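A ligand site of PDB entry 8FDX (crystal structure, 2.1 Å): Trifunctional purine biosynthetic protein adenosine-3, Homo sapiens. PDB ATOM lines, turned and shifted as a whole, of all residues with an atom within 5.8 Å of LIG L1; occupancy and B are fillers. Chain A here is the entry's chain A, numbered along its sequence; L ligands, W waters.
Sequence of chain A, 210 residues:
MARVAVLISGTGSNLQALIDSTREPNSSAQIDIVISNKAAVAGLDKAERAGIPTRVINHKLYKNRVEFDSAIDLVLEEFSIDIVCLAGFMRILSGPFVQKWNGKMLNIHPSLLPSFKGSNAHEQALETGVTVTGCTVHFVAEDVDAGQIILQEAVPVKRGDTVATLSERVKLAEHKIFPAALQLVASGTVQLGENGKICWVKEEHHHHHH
A nitrogen (N1) of LIG L1 is in hydrogen-bond range of the backbone carbonyl oxygen of Leu 93 (3.1 Å). The backbone carbonyl oxygen (O) of Glu 142 sits at hydrogen-bond distance from a nitrogen (N1) of LIG L1 (2.7 Å). O1 of LIG L1 sits at hydrogen-bond distance from N of Asp 145 (2.9 Å). The guanidinium group of Arg 91 is in salt-bridge range of an oxygen (O5) of LIG L1. O of Ala 141 sits at hydrogen-bond distance from N4 of LIG L1, 2.5 Å away. The backbone carbonyl oxygen (O) of Met 90 sits at hydrogen-bond distance from a nitrogen (N2) of LIG L1 (2.7 Å). The backbone NH (N) of Leu 93 is in hydrogen-bond range of a nitrogen (N3) of LIG L1 (3.0 Å). S2 of LIG L1 lies close to N of Ser 119 (3.6 Å). An oxygen (O4) of LIG L1 lies within salt-bridge range of the side-chain amino group of Lys 38 (3.8 Å). NH2 of Arg 65 lies within salt-bridge range of O5 of LIG L1 (3.2 Å). The backbone NH (N) of Ile 92 is in hydrogen-bond range of an oxygen (O6) of LIG L1 (2.9 Å).
The guanidinium group (NH1) of Arg 65 is in hydrogen-bond range of the backbone carbonyl oxygen (O) of Ile 92 (3.0 Å). OD2 of Asp 145 is in hydrogen-bond range of N of Gly 118 (2.9 Å). OD1 of Asn 107 sits close to O of Leu 86, 3.5 Å away. The backbone NH of Asn 107 sits at hydrogen-bond distance from the backbone carbonyl oxygen of His 138 (2.9 Å). ND1 of His 109 lies close to OD2 of Asp 145 (3.5 Å).
Leu 86 touches LIG L1. O of Phe 89 touches C10 of LIG L1 (3.0 Å). Val 98 touches LIG L1. Asn 107 touches LIG L1. C of Gly 118 touches S2 of LIG L1 (3.7 Å). CE1 of His 138 touches O1 of LIG L1, at 3.7 Å. Val 140 touches LIG L1 (CG1 to C14, 3.5 Å). O of Asp 143 touches O1 of LIG L1, at 3.9 Å. Val 144 touches LIG L1 (CA to O1, 3.4 Å). Hydrophobic or aromatic side chains that line LIG L1: Leu 86, Met 90, Ile 92, Leu 93, Val 98, His 138, Val 140 and Val 144.
Water W3 lies within hydrogen-bond range of the side-chain carboxylate (OD1) of Asp 145 (2.5 Å), a ring nitrogen (ND1) of His 109 (2.6 Å), a nitrogen (N2) of LG2 L2 (2.7 Å) and the side-chain amide nitrogen (ND2) of Asn 107 (2.9 Å).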
ATOM      1  N   ASN A  37     -18.375  21.615 -14.831  1.00  0.00           N
ATOM      2  CA  ASN A  37     -17.689  22.774 -14.292  1.00  0.00           C
ATOM      3  C   ASN A  37     -16.722  23.408 -15.304  1.00  0.00           C
ATOM      4  O   ASN A  37     -16.010  24.351 -14.954  1.00  0.00           O
ATOM      5  CB  ASN A  37     -16.940  22.394 -13.013  1.00  0.00           C
ATOM      6  CG  ASN A  37     -15.665  21.609 -13.297  1.00  0.00           C
ATOM      7  OD1 ASN A  37     -15.697  20.591 -13.988  1.00  0.00           O
ATOM      8  ND2 ASN A  37     -14.546  22.096 -12.779  1.00  0.00           N
ATOM      9  N   LYS A  38     -16.718  22.928 -16.557  1.00  0.00           N
ATOM     10  CA  LYS A  38     -15.796  23.393 -17.585  1.00  0.00           C
ATOM     11  C   LYS A  38     -16.508  23.426 -18.924  1.00  0.00           C
ATOM     12  O   LYS A  38     -17.165  22.443 -19.304  1.00  0.00           O
ATOM     13  CB  LYS A  38     -14.558  22.475 -17.683  1.00  0.00           C
ATOM     14  CG  LYS A  38     -13.729  22.399 -16.390  1.00  0.00           C
ATOM     15  CD  LYS A  38     -12.539  21.459 -16.529  1.00  0.00           C
ATOM     16  CE  LYS A  38     -11.656  21.508 -15.284  1.00  0.00           C
ATOM     17  NZ  LYS A  38     -10.561  20.490 -15.340  1.00  0.00           N
ATOM     18  N   ARG A  65     -15.407  27.185  -2.126  1.00  0.00           N
ATOM     19  CA  ARG A  65     -16.038  25.941  -2.534  1.00  0.00           C
ATOM     20  C   ARG A  65     -17.540  25.967  -2.272  1.00  0.00           C
ATOM     21  O   ARG A  65     -18.329  25.525  -3.123  1.00  0.00           O
ATOM     22  CB  ARG A  65     -15.379  24.756  -1.826  1.00  0.00           C
ATOM     23  CG  ARG A  65     -14.276  24.105  -2.654  1.00  0.00           C
ATOM     24  CD  ARG A  65     -13.619  22.896  -1.970  1.00  0.00           C
ATOM     25  NE  ARG A  65     -12.190  22.822  -2.279  1.00  0.00           N
ATOM     26  CZ  ARG A  65     -11.669  22.409  -3.443  1.00  0.00           C
ATOM     27  NH1 ARG A  65     -12.457  21.995  -4.437  1.00  0.00           N
ATOM     28  NH2 ARG A  65     -10.355  22.399  -3.609  1.00  0.00           N
ATOM     29  N   LEU A  86     -21.224  11.649  -9.879  1.00  0.00           N
ATOM     30  CA  LEU A  86     -19.967  12.289 -10.275  1.00  0.00           C
ATOM     31  C   LEU A  86     -19.261  11.394 -11.286  1.00  0.00           C
ATOM     32  O   LEU A  86     -18.707  10.341 -10.926  1.00  0.00           O
ATOM     33  CB  LEU A  86     -19.073  12.550  -9.060  1.00  0.00           C
ATOM     34  CG  LEU A  86     -19.792  13.224  -7.893  1.00  0.00           C
ATOM     35  CD1 LEU A  86     -18.791  13.628  -6.829  1.00  0.00           C
ATOM     36  CD2 LEU A  86     -20.564  14.427  -8.386  1.00  0.00           C
ATOM     37  N   PHE A  89     -16.167  14.082 -12.761  1.00  0.00           N
ATOM     38  CA  PHE A  89     -16.172  15.397 -12.146  1.00  0.00           C
ATOM     39  C   PHE A  89     -15.012  15.499 -11.168  1.00  0.00           C
ATOM     40  O   PHE A  89     -14.830  14.627 -10.309  1.00  0.00           O
ATOM     41  CB  PHE A  89     -17.501  15.621 -11.441  1.00  0.00           C
ATOM     42  CG  PHE A  89     -17.617  16.933 -10.740  1.00  0.00           C
ATOM     43  CD1 PHE A  89     -17.925  18.079 -11.445  1.00  0.00           C
ATOM     44  CD2 PHE A  89     -17.429  17.015  -9.366  1.00  0.00           C
ATOM     45  CE1 PHE A  89     -18.052  19.292 -10.792  1.00  0.00           C
ATOM     46  CE2 PHE A  89     -17.538  18.213  -8.706  1.00  0.00           C
ATOM     47  CZ  PHE A  89     -17.860  19.362  -9.414  1.00  0.00           C
ATOM     48  N   MET A  90     -14.232  16.574 -11.270  1.00  0.00           N
ATOM     49  CA  MET A  90     -12.907  16.606 -10.654  1.00  0.00           C
ATOM     50  C   MET A  90     -12.764  17.589  -9.500  1.00  0.00           C
ATOM     51  O   MET A  90     -11.662  17.720  -8.959  1.00  0.00           O
ATOM     52  CB  MET A  90     -11.844  16.936 -11.721  1.00  0.00           C
ATOM     53  CG  MET A  90     -11.339  15.723 -12.528  1.00  0.00           C
ATOM     54  SD  MET A  90     -11.217  14.128 -11.648  1.00  0.00           S
ATOM     55  CE  MET A  90     -10.132  14.530 -10.269  1.00  0.00           C
ATOM     56  N   ARG A  91     -13.827  18.269  -9.086  1.00  0.00           N
ATOM     57  CA  ARG A  91     -13.732  19.242  -8.007  1.00  0.00           C
ATOM     58  C   ARG A  91     -14.165  18.604  -6.704  1.00  0.00           C
ATOM     59  O   ARG A  91     -15.214  17.950  -6.635  1.00  0.00           O
ATOM     60  CB  ARG A  91     -14.585  20.480  -8.289  1.00  0.00           C
ATOM     61  CG  ARG A  91     -14.365  21.087  -9.665  1.00  0.00           C
ATOM     62  CD  ARG A  91     -13.009  21.800  -9.751  1.00  0.00           C
ATOM     63  NE  ARG A  91     -12.678  22.508  -8.523  1.00  0.00           N
ATOM     64  CZ  ARG A  91     -11.482  23.000  -8.236  1.00  0.00           C
ATOM     65  NH1 ARG A  91     -10.471  22.850  -9.091  1.00  0.00           N
ATOM     66  NH2 ARG A  91     -11.286  23.633  -7.079  1.00  0.00           N
ATOM     67  N   ILE A  92     -13.360  18.785  -5.657  1.00  0.00           N
ATOM     68  CA  ILE A  92     -13.736  18.240  -4.366  1.00  0.00           C
ATOM     69  C   ILE A  92     -14.867  19.079  -3.797  1.00  0.00           C
ATOM     70  O   ILE A  92     -14.851  20.313  -3.862  1.00  0.00           O
ATOM     71  CB  ILE A  92     -12.529  18.219  -3.423  1.00  0.00           C
ATOM     72  CG1 ILE A  92     -11.447  17.305  -4.003  1.00  0.00           C
ATOM     73  CG2 ILE A  92     -12.943  17.686  -2.061  1.00  0.00           C
ATOM     74  CD1 ILE A  92     -10.109  17.419  -3.321  1.00  0.00           C
ATOM     75  N   LEU A  93     -15.875  18.409  -3.261  1.00  0.00           N
ATOM     76  CA  LEU A  93     -17.086  19.068  -2.820  1.00  0.00           C
ATOM     77  C   LEU A  93     -17.012  19.406  -1.334  1.00  0.00           C
ATOM     78  O   LEU A  93     -16.368  18.698  -0.552  1.00  0.00           O
ATOM     79  CB  LEU A  93     -18.305  18.199  -3.114  1.00  0.00           C
ATOM     80  CG  LEU A  93     -18.460  17.919  -4.608  1.00  0.00           C
ATOM     81  CD1 LEU A  93     -19.461  16.819  -4.908  1.00  0.00           C
ATOM     82  CD2 LEU A  93     -18.850  19.204  -5.313  1.00  0.00           C
ATOM     83  N   SER A  94     -17.694  20.494  -0.963  1.00  0.00           N
ATOM     84  CA  SER A  94     -17.671  20.994   0.409  1.00  0.00           C
ATOM     85  C   SER A  94     -18.527  20.132   1.323  1.00  0.00           C
ATOM     86  O   SER A  94     -19.507  19.500   0.892  1.00  0.00           O
ATOM     87  CB  SER A  94     -18.168  22.441   0.463  1.00  0.00           C
ATOM     88  OG  SER A  94     -19.587  22.521   0.436  1.00  0.00           O
ATOM     89  N   GLY A  95     -18.158  20.117   2.595  1.00  0.00           N
ATOM     90  CA  GLY A  95     -18.867  19.398   3.625  1.00  0.00           C
ATOM     91  C   GLY A  95     -20.376  19.542   3.635  1.00  0.00           C
ATOM     92  O   GLY A  95     -21.101  18.539   3.627  1.00  0.00           O
ATOM     93  N   VAL A  98     -21.971  17.808   0.713  1.00  0.00           N
ATOM     94  CA  VAL A  98     -21.917  16.351   0.839  1.00  0.00           C
ATOM     95  C   VAL A  98     -22.898  15.857   1.882  1.00  0.00           C
ATOM     96  O   VAL A  98     -23.550  14.815   1.706  1.00  0.00           O
ATOM     97  CB  VAL A  98     -20.473  15.903   1.153  1.00  0.00           C
ATOM     98  CG1 VAL A  98     -20.457  14.412   1.458  1.00  0.00           C
ATOM     99  CG2 VAL A  98     -19.553  16.237  -0.022  1.00  0.00           C
ATOM    100  N   ASN A 107     -19.884   8.380  -6.801  1.00  0.00           N
ATOM    101  CA  ASN A 107     -18.662   8.726  -7.508  1.00  0.00           C
ATOM    102  C   ASN A 107     -18.055   7.470  -8.107  1.00  0.00           C
ATOM    103  O   ASN A 107     -18.147   6.386  -7.514  1.00  0.00           O
ATOM    104  CB  ASN A 107     -17.669   9.387  -6.572  1.00  0.00           C
ATOM    105  CG  ASN A 107     -16.383   9.723  -7.274  1.00  0.00           C
ATOM    106  OD1 ASN A 107     -16.398  10.349  -8.329  1.00  0.00           O
ATOM    107  ND2 ASN A 107     -15.266   9.288  -6.707  1.00  0.00           N
ATOM    108  N   HIS A 109     -14.443   5.934  -9.279  1.00  0.00           N
ATOM    109  CA  HIS A 109     -13.028   6.164  -9.036  1.00  0.00           C
ATOM    110  C   HIS A 109     -12.229   5.050  -9.691  1.00  0.00           C
ATOM    111  O   HIS A 109     -12.528   3.855  -9.468  1.00  0.00           O
ATOM    112  CB  HIS A 109     -12.726   6.237  -7.525  1.00  0.00           C
ATOM    113  CG  HIS A 109     -11.285   6.533  -7.233  1.00  0.00           C
ATOM    114  ND1 HIS A 109     -10.748   7.797  -7.318  1.00  0.00           N
ATOM    115  CD2 HIS A 109     -10.267   5.721  -6.865  1.00  0.00           C
ATOM    116  CE1 HIS A 109      -9.457   7.755  -7.006  1.00  0.00           C
ATOM    117  NE2 HIS A 109      -9.149   6.506  -6.719  1.00  0.00           N
ATOM    118  N   GLY A 118      -7.268   9.695  -4.746  1.00  0.00           N
ATOM    119  CA  GLY A 118      -6.720  10.891  -5.357  1.00  0.00           C
ATOM    120  C   GLY A 118      -6.874  10.935  -6.865  1.00  0.00           C
ATOM    121  O   GLY A 118      -7.546  10.102  -7.491  1.00  0.00           O
ATOM    122  N   SER A 119      -6.211  11.916  -7.455  1.00  0.00           N
ATOM    123  CA  SER A 119      -6.538  12.359  -8.813  1.00  0.00           C
ATOM    124  C   SER A 119      -5.839  11.570  -9.915  1.00  0.00           C
ATOM    125  O   SER A 119      -6.215  11.713 -11.088  1.00  0.00           O
ATOM    126  CB  SER A 119      -6.181  13.841  -8.964  1.00  0.00           C
ATOM    127  OG  SER A 119      -4.889  14.066  -8.433  1.00  0.00           O
ATOM    128  N   HIS A 138     -18.641   4.425  -5.268  1.00  0.00           N
ATOM    129  CA  HIS A 138     -18.895   4.565  -3.852  1.00  0.00           C
ATOM    130  C   HIS A 138     -19.809   5.756  -3.624  1.00  0.00           C
ATOM    131  O   HIS A 138     -19.839   6.689  -4.444  1.00  0.00           O
ATOM    132  CB  HIS A 138     -17.617   4.759  -3.068  1.00  0.00           C
ATOM    133  CG  HIS A 138     -16.852   5.972  -3.472  1.00  0.00           C
ATOM    134  ND1 HIS A 138     -16.963   7.186  -2.830  1.00  0.00           N
ATOM    135  CD2 HIS A 138     -15.968   6.158  -4.481  1.00  0.00           C
ATOM    136  CE1 HIS A 138     -16.181   8.073  -3.413  1.00  0.00           C
ATOM    137  NE2 HIS A 138     -15.555   7.475  -4.420  1.00  0.00           N
ATOM    138  N   PHE A 139     -20.556   5.704  -2.535  1.00  0.00           N
ATOM    139  CA  PHE A 139     -21.253   6.892  -2.045  1.00  0.00           C
ATOM    140  C   PHE A 139     -20.245   7.970  -1.683  1.00  0.00           C
ATOM    141  O   PHE A 139     -19.176   7.687  -1.133  1.00  0.00           O
ATOM    142  CB  PHE A 139     -22.099   6.539  -0.813  1.00  0.00           C
ATOM    143  CG  PHE A 139     -23.388   5.893  -1.169  1.00  0.00           C
ATOM    144  CD1 PHE A 139     -24.341   6.586  -1.877  1.00  0.00           C
ATOM    145  CD2 PHE A 139     -23.646   4.580  -0.806  1.00  0.00           C
ATOM    146  CE1 PHE A 139     -25.543   5.993  -2.204  1.00  0.00           C
ATOM    147  CE2 PHE A 139     -24.832   3.988  -1.145  1.00  0.00           C
ATOM    148  CZ  PHE A 139     -25.787   4.687  -1.836  1.00  0.00           C
ATOM    149  N   VAL A 140     -20.571   9.220  -1.997  1.00  0.00           N
ATOM    150  CA  VAL A 140     -19.650  10.303  -1.676  1.00  0.00           C
ATOM    151  C   VAL A 140     -19.809  10.644  -0.199  1.00  0.00           C
ATOM    152  O   VAL A 140     -20.911  10.983   0.261  1.00  0.00           O
ATOM    153  CB  VAL A 140     -19.899  11.522  -2.558  1.00  0.00           C
ATOM    154  CG1 VAL A 140     -18.993  12.664  -2.124  1.00  0.00           C
ATOM    155  CG2 VAL A 140     -19.641  11.181  -4.012  1.00  0.00           C
ATOM    156  N   ALA A 141     -18.723  10.537   0.545  1.00  0.00           N
ATOM    157  CA  ALA A 141     -18.682  11.074   1.895  1.00  0.00           C
ATOM    158  C   ALA A 141     -17.752  12.270   1.911  1.00  0.00           C
ATOM    159  O   ALA A 141     -17.120  12.620   0.901  1.00  0.00           O
ATOM    160  CB  ALA A 141     -18.245   9.990   2.900  1.00  0.00           C
ATOM    161  N   GLU A 142     -17.671  12.944   3.062  1.00  0.00           N
ATOM    162  CA  GLU A 142     -16.863  14.162   3.094  1.00  0.00           C
ATOM    163  C   GLU A 142     -15.397  13.843   2.832  1.00  0.00           C
ATOM    164  O   GLU A 142     -14.724  14.510   2.035  1.00  0.00           O
ATOM    165  CB  GLU A 142     -17.030  14.885   4.422  1.00  0.00           C
ATOM    166  CG  GLU A 142     -16.687  16.358   4.302  1.00  0.00           C
ATOM    167  CD  GLU A 142     -17.020  17.138   5.563  1.00  0.00           C
ATOM    168  OE1 GLU A 142     -16.091  17.767   6.118  1.00  0.00           O
ATOM    169  OE2 GLU A 142     -18.192  17.102   5.997  1.00  0.00           O
ATOM    170  N   ASP A 143     -14.893  12.809   3.504  1.00  0.00           N
ATOM    171  CA  ASP A 143     -13.547  12.300   3.254  1.00  0.00           C
ATOM    172  C   ASP A 143     -13.413  11.765   1.825  1.00  0.00           C
ATOM    173  O   ASP A 143     -14.028  10.757   1.470  1.00  0.00           O
ATOM    174  CB  ASP A 143     -13.246  11.224   4.291  1.00  0.00           C
ATOM    175  CG  ASP A 143     -11.763  10.953   4.411  1.00  0.00           C
ATOM    176  OD1 ASP A 143     -10.979  11.794   3.935  1.00  0.00           O
ATOM    177  OD2 ASP A 143     -11.407   9.890   4.979  1.00  0.00           O
ATOM    178  N   VAL A 144     -12.590  12.430   1.002  1.00  0.00           N
ATOM    179  CA  VAL A 144     -12.508  12.115  -0.425  1.00  0.00           C
ATOM    180  C   VAL A 144     -12.180  10.638  -0.635  1.00  0.00           C
ATOM    181  O   VAL A 144     -11.284  10.088   0.020  1.00  0.00           O
ATOM    182  CB  VAL A 144     -11.461  13.006  -1.096  1.00  0.00           C
ATOM    183  CG1 VAL A 144     -11.423  12.766  -2.601  1.00  0.00           C
ATOM    184  CG2 VAL A 144     -11.773  14.459  -0.791  1.00  0.00           C
ATOM    185  N   ASP A 145     -12.912   9.987  -1.552  1.00  0.00           N
ATOM    186  CA  ASP A 145     -12.663   8.601  -1.964  1.00  0.00           C
ATOM    187  C   ASP A 145     -12.731   7.634  -0.784  1.00  0.00           C
ATOM    188  O   ASP A 145     -12.053   6.591  -0.786  1.00  0.00           O
ATOM    189  CB  ASP A 145     -11.311   8.451  -2.679  1.00  0.00           C
ATOM    190  CG  ASP A 145     -11.241   9.263  -3.967  1.00  0.00           C
ATOM    191  OD1 ASP A 145     -12.306   9.586  -4.542  1.00  0.00           O
ATOM    192  OD2 ASP A 145     -10.102   9.571  -4.402  1.00  0.00           O
ATOM    193  N   ALA A 146     -13.531   7.954   0.234  1.00  0.00           N
ATOM    194  CA  ALA A 146     -13.653   7.106   1.400  1.00  0.00           C
ATOM    195  C   ALA A 146     -15.093   6.752   1.750  1.00  0.00           C
ATOM    196  O   ALA A 146     -15.312   6.001   2.704  1.00  0.00           O
ATOM    197  CB  ALA A 146     -12.996   7.759   2.626  1.00  0.00           C
ATOM    198  N   GLY A 147     -16.077   7.260   1.008  1.00  0.00           N
ATOM    199  CA  GLY A 147     -17.447   6.847   1.220  1.00  0.00           C
ATOM    200  C   GLY A 147     -17.642   5.346   1.047  1.00  0.00           C
ATOM    201  O   GLY A 147     -16.760   4.599   0.623  1.00  0.00           O
HETATM  202  O1  LIG L   1     -15.344  11.438  -2.184  1.00  0.00           O
HETATM  203  N1  LIG L   1     -16.107  15.646   0.013  1.00  0.00           N
HETATM  204  C1  LIG L   1     -10.852  15.082  -6.956  1.00  0.00           C
HETATM  205  C2  LIG L   1     -10.144  12.973  -6.119  1.00  0.00           C
HETATM  206  C3  LIG L   1      -8.770  16.710  -6.931  1.00  0.00           C
HETATM  207  O2  LIG L   1      -7.604  16.796  -6.723  1.00  0.00           O
HETATM  208  N2  LIG L   1      -9.520  17.871  -7.342  1.00  0.00           N
HETATM  209  C4  LIG L   1      -8.860  19.153  -7.529  1.00  0.00           C
HETATM  210  C5  LIG L   1      -8.997  19.632  -8.976  1.00  0.00           C
HETATM  211  C6  LIG L   1      -8.095  18.849  -9.930  1.00  0.00           C
HETATM  212  C7  LIG L   1      -8.657  18.786 -11.362  1.00  0.00           C
HETATM  213  O3  LIG L   1      -8.363  17.808 -12.116  1.00  0.00           O
HETATM  214  O4  LIG L   1      -9.409  19.707 -11.786  1.00  0.00           O
HETATM  215  C8  LIG L   1      -9.533  20.135  -6.567  1.00  0.00           C
HETATM  216  O5  LIG L   1      -8.873  21.089  -6.074  1.00  0.00           O
HETATM  217  O6  LIG L   1     -10.752  19.991  -6.237  1.00  0.00           O
HETATM  218  C9  LIG L   1     -14.993  13.248  -7.405  1.00  0.00           C
HETATM  219  C10 LIG L   1     -13.588  13.794  -7.712  1.00  0.00           C
HETATM  220  C11 LIG L   1     -12.606  13.114  -6.774  1.00  0.00           C
HETATM  221  C12 LIG L   1     -11.214  13.733  -6.629  1.00  0.00           C
HETATM  222  C13 LIG L   1     -15.887  14.844  -1.167  1.00  0.00           C
HETATM  223  C14 LIG L   1     -15.478  12.618  -2.247  1.00  0.00           C
HETATM  224  C15 LIG L   1     -15.213  12.643  -4.846  1.00  0.00           C
HETATM  225  C16 LIG L   1     -15.229  13.535  -5.925  1.00  0.00           C
HETATM  226  C17 LIG L   1     -15.439  13.310  -3.579  1.00  0.00           C
HETATM  227  C18 LIG L   1     -15.602  14.693  -3.663  1.00  0.00           C
HETATM  228  C19 LIG L   1      -9.494  15.387  -6.719  1.00  0.00           C
HETATM  229  N3  LIG L   1     -15.832  15.500  -2.461  1.00  0.00           N
HETATM  230  N4  LIG L   1     -15.709  13.401  -1.068  1.00  0.00           N
HETATM  231  S1  LIG L   1     -15.491  15.082  -5.292  1.00  0.00           S
HETATM  232  S2  LIG L   1      -8.785  13.986  -6.088  1.00  0.00           S
HETATM  233  C1  LG2 L   2     -12.798   8.204 -15.322  1.00  0.00           C
HETATM  234  O1  LG2 L   2     -11.778   7.188 -15.417  1.00  0.00           O
HETATM  235  C2  LG2 L   2     -13.077   8.448 -13.857  1.00  0.00           C
HETATM  236  O2  LG2 L   2     -13.036   7.254 -13.054  1.00  0.00           O
HETATM  237  C3  LG2 L   2     -11.922   9.372 -13.508  1.00  0.00           C
HETATM  238  O3  LG2 L   2     -11.777  10.216 -14.640  1.00  0.00           O
HETATM  239  C4  LG2 L   2     -12.225   9.524 -15.806  1.00  0.00           C
HETATM  240  C5  LG2 L   2     -13.266  10.375 -16.501  1.00  0.00           C
HETATM  241  O4  LG2 L   2     -13.628   9.819 -17.757  1.00  0.00           O
HETATM  242  N1  LG2 L   2     -12.235  10.171 -12.343  1.00  0.00           N
HETATM  243  C6  LG2 L   2     -11.354  10.302 -11.368  1.00  0.00           C
HETATM  244  O5  LG2 L   2     -10.133  10.204 -11.522  1.00  0.00           O
HETATM  245  C7  LG2 L   2     -11.980  10.579 -10.012  1.00  0.00           C
HETATM  246  N2  LG2 L   2     -10.988  10.972  -9.038  1.00  0.00           N
HETATM  247  P1  LG2 L   2     -14.961  10.319 -18.522  1.00  0.00           P
HETATM  248  O6  LG2 L   2     -16.112   9.679 -17.760  1.00  0.00           O
HETATM  249  O7  LG2 L   2     -14.762   9.767 -19.926  1.00  0.00           O
HETATM  250  O8  LG2 L   2     -14.960  11.830 -18.392  1.00  0.00           O
HETATM  251  O   HOH W   1     -16.096   9.689  -0.145  1.00  0.00           O
HETATM  252  O   HOH W   2     -15.824  12.189 -10.373  1.00  0.00           O
HETATM  253  O   HOH W   3     -12.424   9.767  -7.031  1.00  0.00           O
HETATM  254  O   HOH W   4      -8.069  15.471 -14.515  1.00  0.00           O
